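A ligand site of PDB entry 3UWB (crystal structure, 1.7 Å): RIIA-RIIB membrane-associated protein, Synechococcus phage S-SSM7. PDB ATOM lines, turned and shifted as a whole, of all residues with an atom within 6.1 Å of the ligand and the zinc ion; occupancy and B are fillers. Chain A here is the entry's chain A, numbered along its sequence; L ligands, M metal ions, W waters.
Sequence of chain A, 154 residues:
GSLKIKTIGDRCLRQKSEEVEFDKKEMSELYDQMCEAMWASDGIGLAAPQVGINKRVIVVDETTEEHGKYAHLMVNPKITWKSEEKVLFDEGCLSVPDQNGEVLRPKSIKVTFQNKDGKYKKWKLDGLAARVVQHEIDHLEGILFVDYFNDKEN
Residues that only touch the ligand: Gly 43, Phe 89, Arg 131, Glu 91 and Asp 42. Hydrophobic or aromatic side chains within 4 Å of the ligand: Ile 44, Phe 89, Leu 94, His 135 and His 139. Within 4 Å of the ligand: Asp 42, Gly 43, Ile 44, Gly 45, Gln 50, Phe 89, Asp 90, Glu 91, Gly 92, Cys 93, Leu 94, Arg 131, His 135, Glu 136 and His 139. The nearest printed residue that does not touch the ligand is Leu 46 (4.1 Å).
The backbone NH of Ala 47 sits at hydrogen-bond distance from the side-chain carboxylate of Glu 136, 3.4 Å away. A ring nitrogen (NE2) of His 139 lies close to the side-chain amide nitrogen (NE2) of Gln 50, 3.4 Å away. OE2 of Glu 136 lies within hydrogen-bond range of N of Leu 46 (3.3 Å). SG of Cys 93 sits close to N of Ser 95 (3.4 Å). The side-chain carboxylate (OE2) of Glu 91 is in salt-bridge range of the guanidinium group (NH1) of Arg 131 (2.8 Å). The side-chain carboxylate of Glu 91 lies within salt-bridge range of the guanidinium group of Arg 105, at 2.9 Å. A ring nitrogen (ND1) of His 135 sits at hydrogen-bond distance from the side-chain carboxylate of Glu 91, 2.8 Å away. The side-chain amide oxygen (OE1) of Gln 50 sits at hydrogen-bond distance from the backbone NH (N) of Ala 47, 2.8 Å away.
Residues that only touch the zinc ion: Gln 50 (3.3 Å). Within 4 Å of the zinc ion: Gln 50, Cys 93, His 135 and His 139.
O4 of the ligand lies within hydrogen-bond range of N of Gly 92. The backbone carbonyl oxygen (O) of Asp 90 sits at hydrogen-bond distance from an oxygen (O5) of the ligand (2.6 Å). The side-chain carboxylate (OE2) of Glu 136 is in hydrogen-bond range of a nitrogen (N1) of the ligand, 2.7 Å away. The side-chain amide oxygen (OE1) of Gln 50 sits at hydrogen-bond distance from a nitrogen (N1) of the ligand, 3.5 Å away. A nitrogen (N1) of the ligand lies within hydrogen-bond range of the backbone carbonyl oxygen of Gly 45, at 3.2 Å. The backbone NH (N) of Ile 44 is in hydrogen-bond range of an oxygen (O3) of the ligand, at 2.8 Å. An oxygen (O1) of the ligand lies close to the backbone NH (N) of Leu 94 (2.9 Å). The backbone carbonyl oxygen (O) of Gly 92 is in hydrogen-bond range of a nitrogen (N2) of the ligand (3.1 Å).
The zinc ion is bound by a ring nitrogen (NE2) of His 135 (2.1 Å), a ring nitrogen (NE2) of His 139 (2.1 Å), an oxygen (O2) of the ligand (2.1 Å), an oxygen (O1) of the ligand (2.2 Å) and the side-chain sulfur (SG) of Cys 93 (2.3 Å). The zinc ion has five donor atoms within binding distance.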
ATOM      1  N   SER A  41      20.725  14.435 -24.457  1.00  0.00           N
ATOM      2  CA  SER A  41      21.243  15.772 -24.769  1.00  0.00           C
ATOM      3  C   SER A  41      22.423  16.167 -23.876  1.00  0.00           C
ATOM      4  O   SER A  41      22.760  17.349 -23.797  1.00  0.00           O
ATOM      5  CB  SER A  41      20.115  16.799 -24.660  1.00  0.00           C
ATOM      6  OG  SER A  41      19.250  16.692 -25.797  1.00  0.00           O
ATOM      7  N   ASP A  42      23.085  15.182 -23.255  1.00  0.00           N
ATOM      8  CA  ASP A  42      24.254  15.437 -22.389  1.00  0.00           C
ATOM      9  C   ASP A  42      24.010  16.408 -21.203  1.00  0.00           C
ATOM     10  O   ASP A  42      24.939  17.115 -20.739  1.00  0.00           O
ATOM     11  CB  ASP A  42      25.456  15.850 -23.244  1.00  0.00           C
ATOM     12  CG  ASP A  42      25.822  14.783 -24.278  1.00  0.00           C
ATOM     13  OD1 ASP A  42      25.788  13.587 -23.951  1.00  0.00           O
ATOM     14  OD2 ASP A  42      26.119  15.155 -25.408  1.00  0.00           O
ATOM     15  N   GLY A  43      22.785  16.394 -20.684  1.00  0.00           N
ATOM     16  CA  GLY A  43      22.474  17.240 -19.578  1.00  0.00           C
ATOM     17  C   GLY A  43      22.744  16.548 -18.265  1.00  0.00           C
ATOM     18  O   GLY A  43      22.950  15.327 -18.193  1.00  0.00           O
ATOM     19  N   ILE A  44      22.775  17.363 -17.214  1.00  0.00           N
ATOM     20  CA  ILE A  44      23.014  16.864 -15.867  1.00  0.00           C
ATOM     21  C   ILE A  44      21.888  17.153 -14.887  1.00  0.00           C
ATOM     22  O   ILE A  44      21.976  16.809 -13.689  1.00  0.00           O
ATOM     23  CB  ILE A  44      24.376  17.375 -15.313  1.00  0.00           C
ATOM     24  CG1 ILE A  44      24.412  18.863 -15.119  1.00  0.00           C
ATOM     25  CG2 ILE A  44      25.552  16.890 -16.183  1.00  0.00           C
ATOM     26  CD1 ILE A  44      25.616  19.296 -14.253  1.00  0.00           C
ATOM     27  N   GLY A  45      20.838  17.777 -15.396  1.00  0.00           N
ATOM     28  CA  GLY A  45      19.588  17.949 -14.696  1.00  0.00           C
ATOM     29  C   GLY A  45      18.481  18.229 -15.710  1.00  0.00           C
ATOM     30  O   GLY A  45      18.744  18.517 -16.895  1.00  0.00           O
ATOM     31  N   LEU A  46      17.236  18.118 -15.269  1.00  0.00           N
ATOM     32  CA  LEU A  46      16.081  18.452 -16.083  1.00  0.00           C
ATOM     33  C   LEU A  46      14.869  18.739 -15.240  1.00  0.00           C
ATOM     34  O   LEU A  46      14.743  18.169 -14.156  1.00  0.00           O
ATOM     35  CB  LEU A  46      15.733  17.335 -17.097  1.00  0.00           C
ATOM     36  CG  LEU A  46      14.972  17.733 -18.385  1.00  0.00           C
ATOM     37  CD1 LEU A  46      15.889  18.510 -19.367  1.00  0.00           C
ATOM     38  CD2 LEU A  46      14.411  16.494 -19.115  1.00  0.00           C
ATOM     39  N   ALA A  47      14.023  19.659 -15.704  1.00  0.00           N
ATOM     40  CA  ALA A  47      12.803  20.023 -15.005  1.00  0.00           C
ATOM     41  C   ALA A  47      11.627  19.743 -15.917  1.00  0.00           C
ATOM     42  O   ALA A  47      11.680  20.014 -17.131  1.00  0.00           O
ATOM     43  CB  ALA A  47      12.829  21.516 -14.578  1.00  0.00           C
ATOM     44  N   GLN A  50      10.424  21.920 -18.872  1.00  0.00           N
ATOM     45  CA  GLN A  50      11.244  21.908 -20.090  1.00  0.00           C
ATOM     46  C   GLN A  50      10.772  20.919 -21.137  1.00  0.00           C
ATOM     47  O   GLN A  50      11.178  21.029 -22.313  1.00  0.00           O
ATOM     48  CB  GLN A  50      12.708  21.572 -19.743  1.00  0.00           C
ATOM     49  CG  GLN A  50      13.427  22.602 -18.884  1.00  0.00           C
ATOM     50  CD  GLN A  50      14.839  22.135 -18.650  1.00  0.00           C
ATOM     51  OE1 GLN A  50      15.084  21.319 -17.756  1.00  0.00           O
ATOM     52  NE2 GLN A  50      15.779  22.582 -19.513  1.00  0.00           N
ATOM     53  N   PHE A  89      29.436  30.226 -11.310  1.00  0.00           N
ATOM     54  CA  PHE A  89      29.556  29.016 -12.152  1.00  0.00           C
ATOM     55  C   PHE A  89      28.950  29.267 -13.526  1.00  0.00           C
ATOM     56  O   PHE A  89      27.913  29.951 -13.652  1.00  0.00           O
ATOM     57  CB  PHE A  89      28.912  27.819 -11.452  1.00  0.00           C
ATOM     58  CG  PHE A  89      29.332  26.478 -12.006  1.00  0.00           C
ATOM     59  CD1 PHE A  89      30.531  25.902 -11.609  1.00  0.00           C
ATOM     60  CD2 PHE A  89      28.549  25.816 -12.920  1.00  0.00           C
ATOM     61  CE1 PHE A  89      30.929  24.667 -12.111  1.00  0.00           C
ATOM     62  CE2 PHE A  89      28.921  24.571 -13.413  1.00  0.00           C
ATOM     63  CZ  PHE A  89      30.117  24.011 -13.008  1.00  0.00           C
ATOM     64  N   ASP A  90      29.636  28.749 -14.563  1.00  0.00           N
ATOM     65  CA  ASP A  90      29.225  28.991 -15.931  1.00  0.00           C
ATOM     66  C   ASP A  90      28.136  27.994 -16.305  1.00  0.00           C
ATOM     67  O   ASP A  90      28.368  26.783 -16.241  1.00  0.00           O
ATOM     68  CB  ASP A  90      30.450  28.783 -16.861  1.00  0.00           C
ATOM     69  CG  ASP A  90      30.231  29.297 -18.269  1.00  0.00           C
ATOM     70  OD1 ASP A  90      29.232  29.949 -18.576  1.00  0.00           O
ATOM     71  OD2 ASP A  90      31.140  29.150 -19.125  1.00  0.00           O
ATOM     72  N   GLU A  91      26.924  28.484 -16.603  1.00  0.00           N
ATOM     73  CA  GLU A  91      25.804  27.594 -16.900  1.00  0.00           C
ATOM     74  C   GLU A  91      25.401  27.657 -18.353  1.00  0.00           C
ATOM     75  O   GLU A  91      25.469  28.705 -19.000  1.00  0.00           O
ATOM     76  CB  GLU A  91      24.564  28.004 -16.091  1.00  0.00           C
ATOM     77  CG  GLU A  91      24.813  28.033 -14.613  1.00  0.00           C
ATOM     78  CD  GLU A  91      23.590  28.251 -13.782  1.00  0.00           C
ATOM     79  OE1 GLU A  91      22.419  28.102 -14.282  1.00  0.00           O
ATOM     80  OE2 GLU A  91      23.768  28.529 -12.581  1.00  0.00           O
ATOM     81  N   GLY A  92      24.905  26.518 -18.848  1.00  0.00           N
ATOM     82  CA  GLY A  92      24.135  26.449 -20.060  1.00  0.00           C
ATOM     83  C   GLY A  92      22.824  25.728 -19.726  1.00  0.00           C
ATOM     84  O   GLY A  92      22.701  25.071 -18.664  1.00  0.00           O
ATOM     85  N   CYS A  93      21.857  25.837 -20.616  1.00  0.00           N
ATOM     86  CA  CYS A  93      20.548  25.268 -20.363  1.00  0.00           C
ATOM     87  C   CYS A  93      20.086  24.599 -21.651  1.00  0.00           C
ATOM     88  O   CYS A  93      20.211  25.196 -22.752  1.00  0.00           O
ATOM     89  CB  CYS A  93      19.528  26.380 -19.984  1.00  0.00           C
ATOM     90  SG  CYS A  93      17.828  25.825 -19.649  1.00  0.00           S
ATOM     91  N   LEU A  94      19.529  23.405 -21.524  1.00  0.00           N
ATOM     92  CA  LEU A  94      19.017  22.691 -22.704  1.00  0.00           C
ATOM     93  C   LEU A  94      17.812  23.406 -23.357  1.00  0.00           C
ATOM     94  O   LEU A  94      17.506  23.144 -24.498  1.00  0.00           O
ATOM     95  CB  LEU A  94      18.687  21.229 -22.312  1.00  0.00           C
ATOM     96  CG  LEU A  94      19.945  20.369 -22.018  1.00  0.00           C
ATOM     97  CD1 LEU A  94      19.439  19.012 -21.556  1.00  0.00           C
ATOM     98  CD2 LEU A  94      20.871  20.248 -23.234  1.00  0.00           C
ATOM     99  N   SER A  95      17.166  24.310 -22.627  1.00  0.00           N
ATOM    100  CA  SER A  95      16.092  25.108 -23.153  1.00  0.00           C
ATOM    101  C   SER A  95      16.569  26.454 -23.711  1.00  0.00           C
ATOM    102  O   SER A  95      15.732  27.246 -24.177  1.00  0.00           O
ATOM    103  CB  SER A  95      14.985  25.273 -22.115  1.00  0.00           C
ATOM    104  OG  SER A  95      14.355  24.035 -21.811  1.00  0.00           O
ATOM    105  N   ARG A 105      25.162  32.060  -7.413  1.00  0.00           N
ATOM    106  CA  ARG A 105      24.163  31.414  -6.571  1.00  0.00           C
ATOM    107  C   ARG A 105      24.803  30.959  -5.260  1.00  0.00           C
ATOM    108  O   ARG A 105      26.013  30.707  -5.189  1.00  0.00           O
ATOM    109  CB  ARG A 105      23.530  30.192  -7.234  1.00  0.00           C
ATOM    110  CG  ARG A 105      23.018  30.369  -8.646  1.00  0.00           C
ATOM    111  CD  ARG A 105      22.300  29.111  -9.088  1.00  0.00           C
ATOM    112  NE  ARG A 105      21.913  29.118 -10.488  1.00  0.00           N
ATOM    113  CZ  ARG A 105      20.696  29.367 -11.001  1.00  0.00           C
ATOM    114  NH1 ARG A 105      19.698  29.755 -10.205  1.00  0.00           N
ATOM    115  NH2 ARG A 105      20.504  29.210 -12.293  1.00  0.00           N
ATOM    116  N   LEU A 128      28.287  20.879  -7.211  1.00  0.00           N
ATOM    117  CA  LEU A 128      27.518  20.792  -8.441  1.00  0.00           C
ATOM    118  C   LEU A 128      26.046  20.420  -8.164  1.00  0.00           C
ATOM    119  O   LEU A 128      25.120  20.980  -8.848  1.00  0.00           O
ATOM    120  CB  LEU A 128      28.157  19.792  -9.389  1.00  0.00           C
ATOM    121  CG  LEU A 128      27.593  19.758 -10.820  1.00  0.00           C
ATOM    122  CD1 LEU A 128      27.705  21.102 -11.541  1.00  0.00           C
ATOM    123  CD2 LEU A 128      28.325  18.702 -11.628  1.00  0.00           C
ATOM    124  N   ARG A 131      24.139  23.417  -7.239  1.00  0.00           N
ATOM    125  CA  ARG A 131      24.013  24.238  -8.408  1.00  0.00           C
ATOM    126  C   ARG A 131      22.882  23.790  -9.331  1.00  0.00           C
ATOM    127  O   ARG A 131      22.050  24.586  -9.779  1.00  0.00           O
ATOM    128  CB  ARG A 131      25.387  24.308  -9.147  1.00  0.00           C
ATOM    129  CG  ARG A 131      25.358  25.007 -10.489  1.00  0.00           C
ATOM    130  CD  ARG A 131      24.822  26.432 -10.414  1.00  0.00           C
ATOM    131  NE  ARG A 131      25.501  27.232  -9.413  1.00  0.00           N
ATOM    132  CZ  ARG A 131      25.996  28.453  -9.595  1.00  0.00           C
ATOM    133  NH1 ARG A 131      25.818  29.058 -10.761  1.00  0.00           N
ATOM    134  NH2 ARG A 131      26.617  29.072  -8.599  1.00  0.00           N
ATOM    135  N   VAL A 132      22.890  22.495  -9.668  1.00  0.00           N
ATOM    136  CA  VAL A 132      21.906  21.902 -10.581  1.00  0.00           C
ATOM    137  C   VAL A 132      20.526  22.089  -9.990  1.00  0.00           C
ATOM    138  O   VAL A 132      19.610  22.502 -10.692  1.00  0.00           O
ATOM    139  CB  VAL A 132      22.209  20.420 -10.892  1.00  0.00           C
ATOM    140  CG1 VAL A 132      21.029  19.809 -11.657  1.00  0.00           C
ATOM    141  CG2 VAL A 132      23.568  20.334 -11.641  1.00  0.00           C
ATOM    142  N   HIS A 135      19.184  25.652 -10.405  1.00  0.00           N
ATOM    143  CA  HIS A 135      18.852  25.885 -11.811  1.00  0.00           C
ATOM    144  C   HIS A 135      17.515  25.260 -12.141  1.00  0.00           C
ATOM    145  O   HIS A 135      16.643  25.851 -12.772  1.00  0.00           O
ATOM    146  CB  HIS A 135      20.011  25.366 -12.700  1.00  0.00           C
ATOM    147  CG  HIS A 135      19.737  25.452 -14.169  1.00  0.00           C
ATOM    148  ND1 HIS A 135      20.423  26.313 -15.008  1.00  0.00           N
ATOM    149  CD2 HIS A 135      18.904  24.715 -14.966  1.00  0.00           C
ATOM    150  CE1 HIS A 135      19.993  26.135 -16.277  1.00  0.00           C
ATOM    151  NE2 HIS A 135      19.062  25.175 -16.264  1.00  0.00           N
ATOM    152  N   GLU A 136      17.318  24.015 -11.720  1.00  0.00           N
ATOM    153  CA  GLU A 136      16.059  23.301 -11.994  1.00  0.00           C
ATOM    154  C   GLU A 136      14.860  23.897 -11.252  1.00  0.00           C
ATOM    155  O   GLU A 136      13.776  23.979 -11.863  1.00  0.00           O
ATOM    156  CB  GLU A 136      16.169  21.809 -11.672  1.00  0.00           C
ATOM    157  CG  GLU A 136      17.319  21.030 -12.346  1.00  0.00           C
ATOM    158  CD  GLU A 136      17.458  21.230 -13.828  1.00  0.00           C
ATOM    159  OE1 GLU A 136      16.464  21.636 -14.510  1.00  0.00           O
ATOM    160  OE2 GLU A 136      18.577  20.985 -14.362  1.00  0.00           O
ATOM    161  N   HIS A 139      13.495  26.777 -13.081  1.00  0.00           N
ATOM    162  CA  HIS A 139      12.585  26.402 -14.162  1.00  0.00           C
ATOM    163  C   HIS A 139      11.160  26.249 -13.687  1.00  0.00           C
ATOM    164  O   HIS A 139      10.213  26.611 -14.443  1.00  0.00           O
ATOM    165  CB  HIS A 139      13.020  25.082 -14.832  1.00  0.00           C
ATOM    166  CG  HIS A 139      14.072  25.235 -15.861  1.00  0.00           C
ATOM    167  ND1 HIS A 139      13.909  25.985 -16.982  1.00  0.00           N
ATOM    168  CD2 HIS A 139      15.349  24.681 -15.933  1.00  0.00           C
ATOM    169  CE1 HIS A 139      15.007  25.891 -17.760  1.00  0.00           C
ATOM    170  NE2 HIS A 139      15.898  25.074 -17.141  1.00  0.00           N
ATOM    171  N   LEU A 144      14.574  31.413 -16.438  1.00  0.00           N
ATOM    172  CA  LEU A 144      15.672  30.952 -17.231  1.00  0.00           C
ATOM    173  C   LEU A 144      16.957  31.665 -16.835  1.00  0.00           C
ATOM    174  O   LEU A 144      16.923  32.832 -16.439  1.00  0.00           O
ATOM    175  CB  LEU A 144      15.400  31.127 -18.733  1.00  0.00           C
ATOM    176  CG  LEU A 144      14.133  30.460 -19.303  1.00  0.00           C
ATOM    177  CD1 LEU A 144      13.888  30.790 -20.786  1.00  0.00           C
ATOM    178  CD2 LEU A 144      14.127  28.944 -19.021  1.00  0.00           C
ATOM    179  N   PHE A 145      18.090  30.967 -16.932  1.00  0.00           N
ATOM    180  CA  PHE A 145      19.311  31.524 -16.344  1.00  0.00           C
ATOM    181  C   PHE A 145      19.710  32.829 -17.011  1.00  0.00           C
ATOM    182  O   PHE A 145      20.360  33.660 -16.413  1.00  0.00           O
ATOM    183  CB  PHE A 145      20.454  30.506 -16.374  1.00  0.00           C
ATOM    184  CG  PHE A 145      21.153  30.404 -17.698  1.00  0.00           C
ATOM    185  CD1 PHE A 145      22.323  31.149 -17.928  1.00  0.00           C
ATOM    186  CD2 PHE A 145      20.632  29.627 -18.743  1.00  0.00           C
ATOM    187  CE1 PHE A 145      22.970  31.064 -19.127  1.00  0.00           C
ATOM    188  CE2 PHE A 145      21.281  29.556 -19.967  1.00  0.00           C
ATOM    189  CZ  PHE A 145      22.434  30.294 -20.138  1.00  0.00           C
HETATM  190  C1  LIG L   1      20.429  21.121 -18.181  1.00  0.00           C
HETATM  191  C2  LIG L   1      19.217  21.960 -17.995  1.00  0.00           C
HETATM  192  O1  LIG L   1      18.929  22.867 -18.773  1.00  0.00           O
HETATM  193  N1  LIG L   1      18.431  21.723 -16.936  1.00  0.00           N
HETATM  194  O2  LIG L   1      17.429  22.669 -16.690  1.00  0.00           O
HETATM  195  C3  LIG L   1      21.657  21.844 -17.594  1.00  0.00           C
HETATM  196  C4  LIG L   1      22.909  21.246 -18.116  1.00  0.00           C
HETATM  197  O3  LIG L   1      23.094  20.022 -18.112  1.00  0.00           O
HETATM  198  C5  LIG L   1      21.650  21.806 -16.078  1.00  0.00           C
HETATM  199  C6  LIG L   1      22.901  22.438 -15.432  1.00  0.00           C
HETATM  200  C7  LIG L   1      22.716  23.847 -15.068  1.00  0.00           C
HETATM  201  C8  LIG L   1      23.617  24.405 -13.925  1.00  0.00           C
HETATM  202  C9  LIG L   1      25.079  24.072 -14.162  1.00  0.00           C
HETATM  203  N2  LIG L   1      23.785  22.183 -18.618  1.00  0.00           N
HETATM  204  C10 LIG L   1      25.137  21.807 -19.039  1.00  0.00           C
HETATM  205  C11 LIG L   1      25.263  22.012 -20.552  1.00  0.00           C
HETATM  206  C12 LIG L   1      26.711  21.871 -21.033  1.00  0.00           C
HETATM  207  C13 LIG L   1      24.318  21.016 -21.247  1.00  0.00           C
HETATM  208  C14 LIG L   1      26.107  22.632 -18.254  1.00  0.00           C
HETATM  209  O4  LIG L   1      25.872  23.797 -18.030  1.00  0.00           O
HETATM  210  N3  LIG L   1      27.288  22.065 -17.855  1.00  0.00           N
HETATM  211  C15 LIG L   1      28.067  22.775 -16.804  1.00  0.00           C
HETATM  212  C16 LIG L   1      27.354  20.590 -17.664  1.00  0.00           C
HETATM  213  C17 LIG L   1      28.618  20.388 -16.803  1.00  0.00           C
HETATM  214  C18 LIG L   1      28.760  21.674 -15.992  1.00  0.00           C
HETATM  215  C19 LIG L   1      29.093  23.681 -17.484  1.00  0.00           C
HETATM  216  O5  LIG L   1      29.749  24.670 -16.620  1.00  0.00           O
HETATM  217 ZN    ZN M   1      17.820  24.480 -17.766  1.00  0.00          ZN
HETATM  218  O   HOH W   1      27.134  18.278 -19.992  1.00  0.00           O
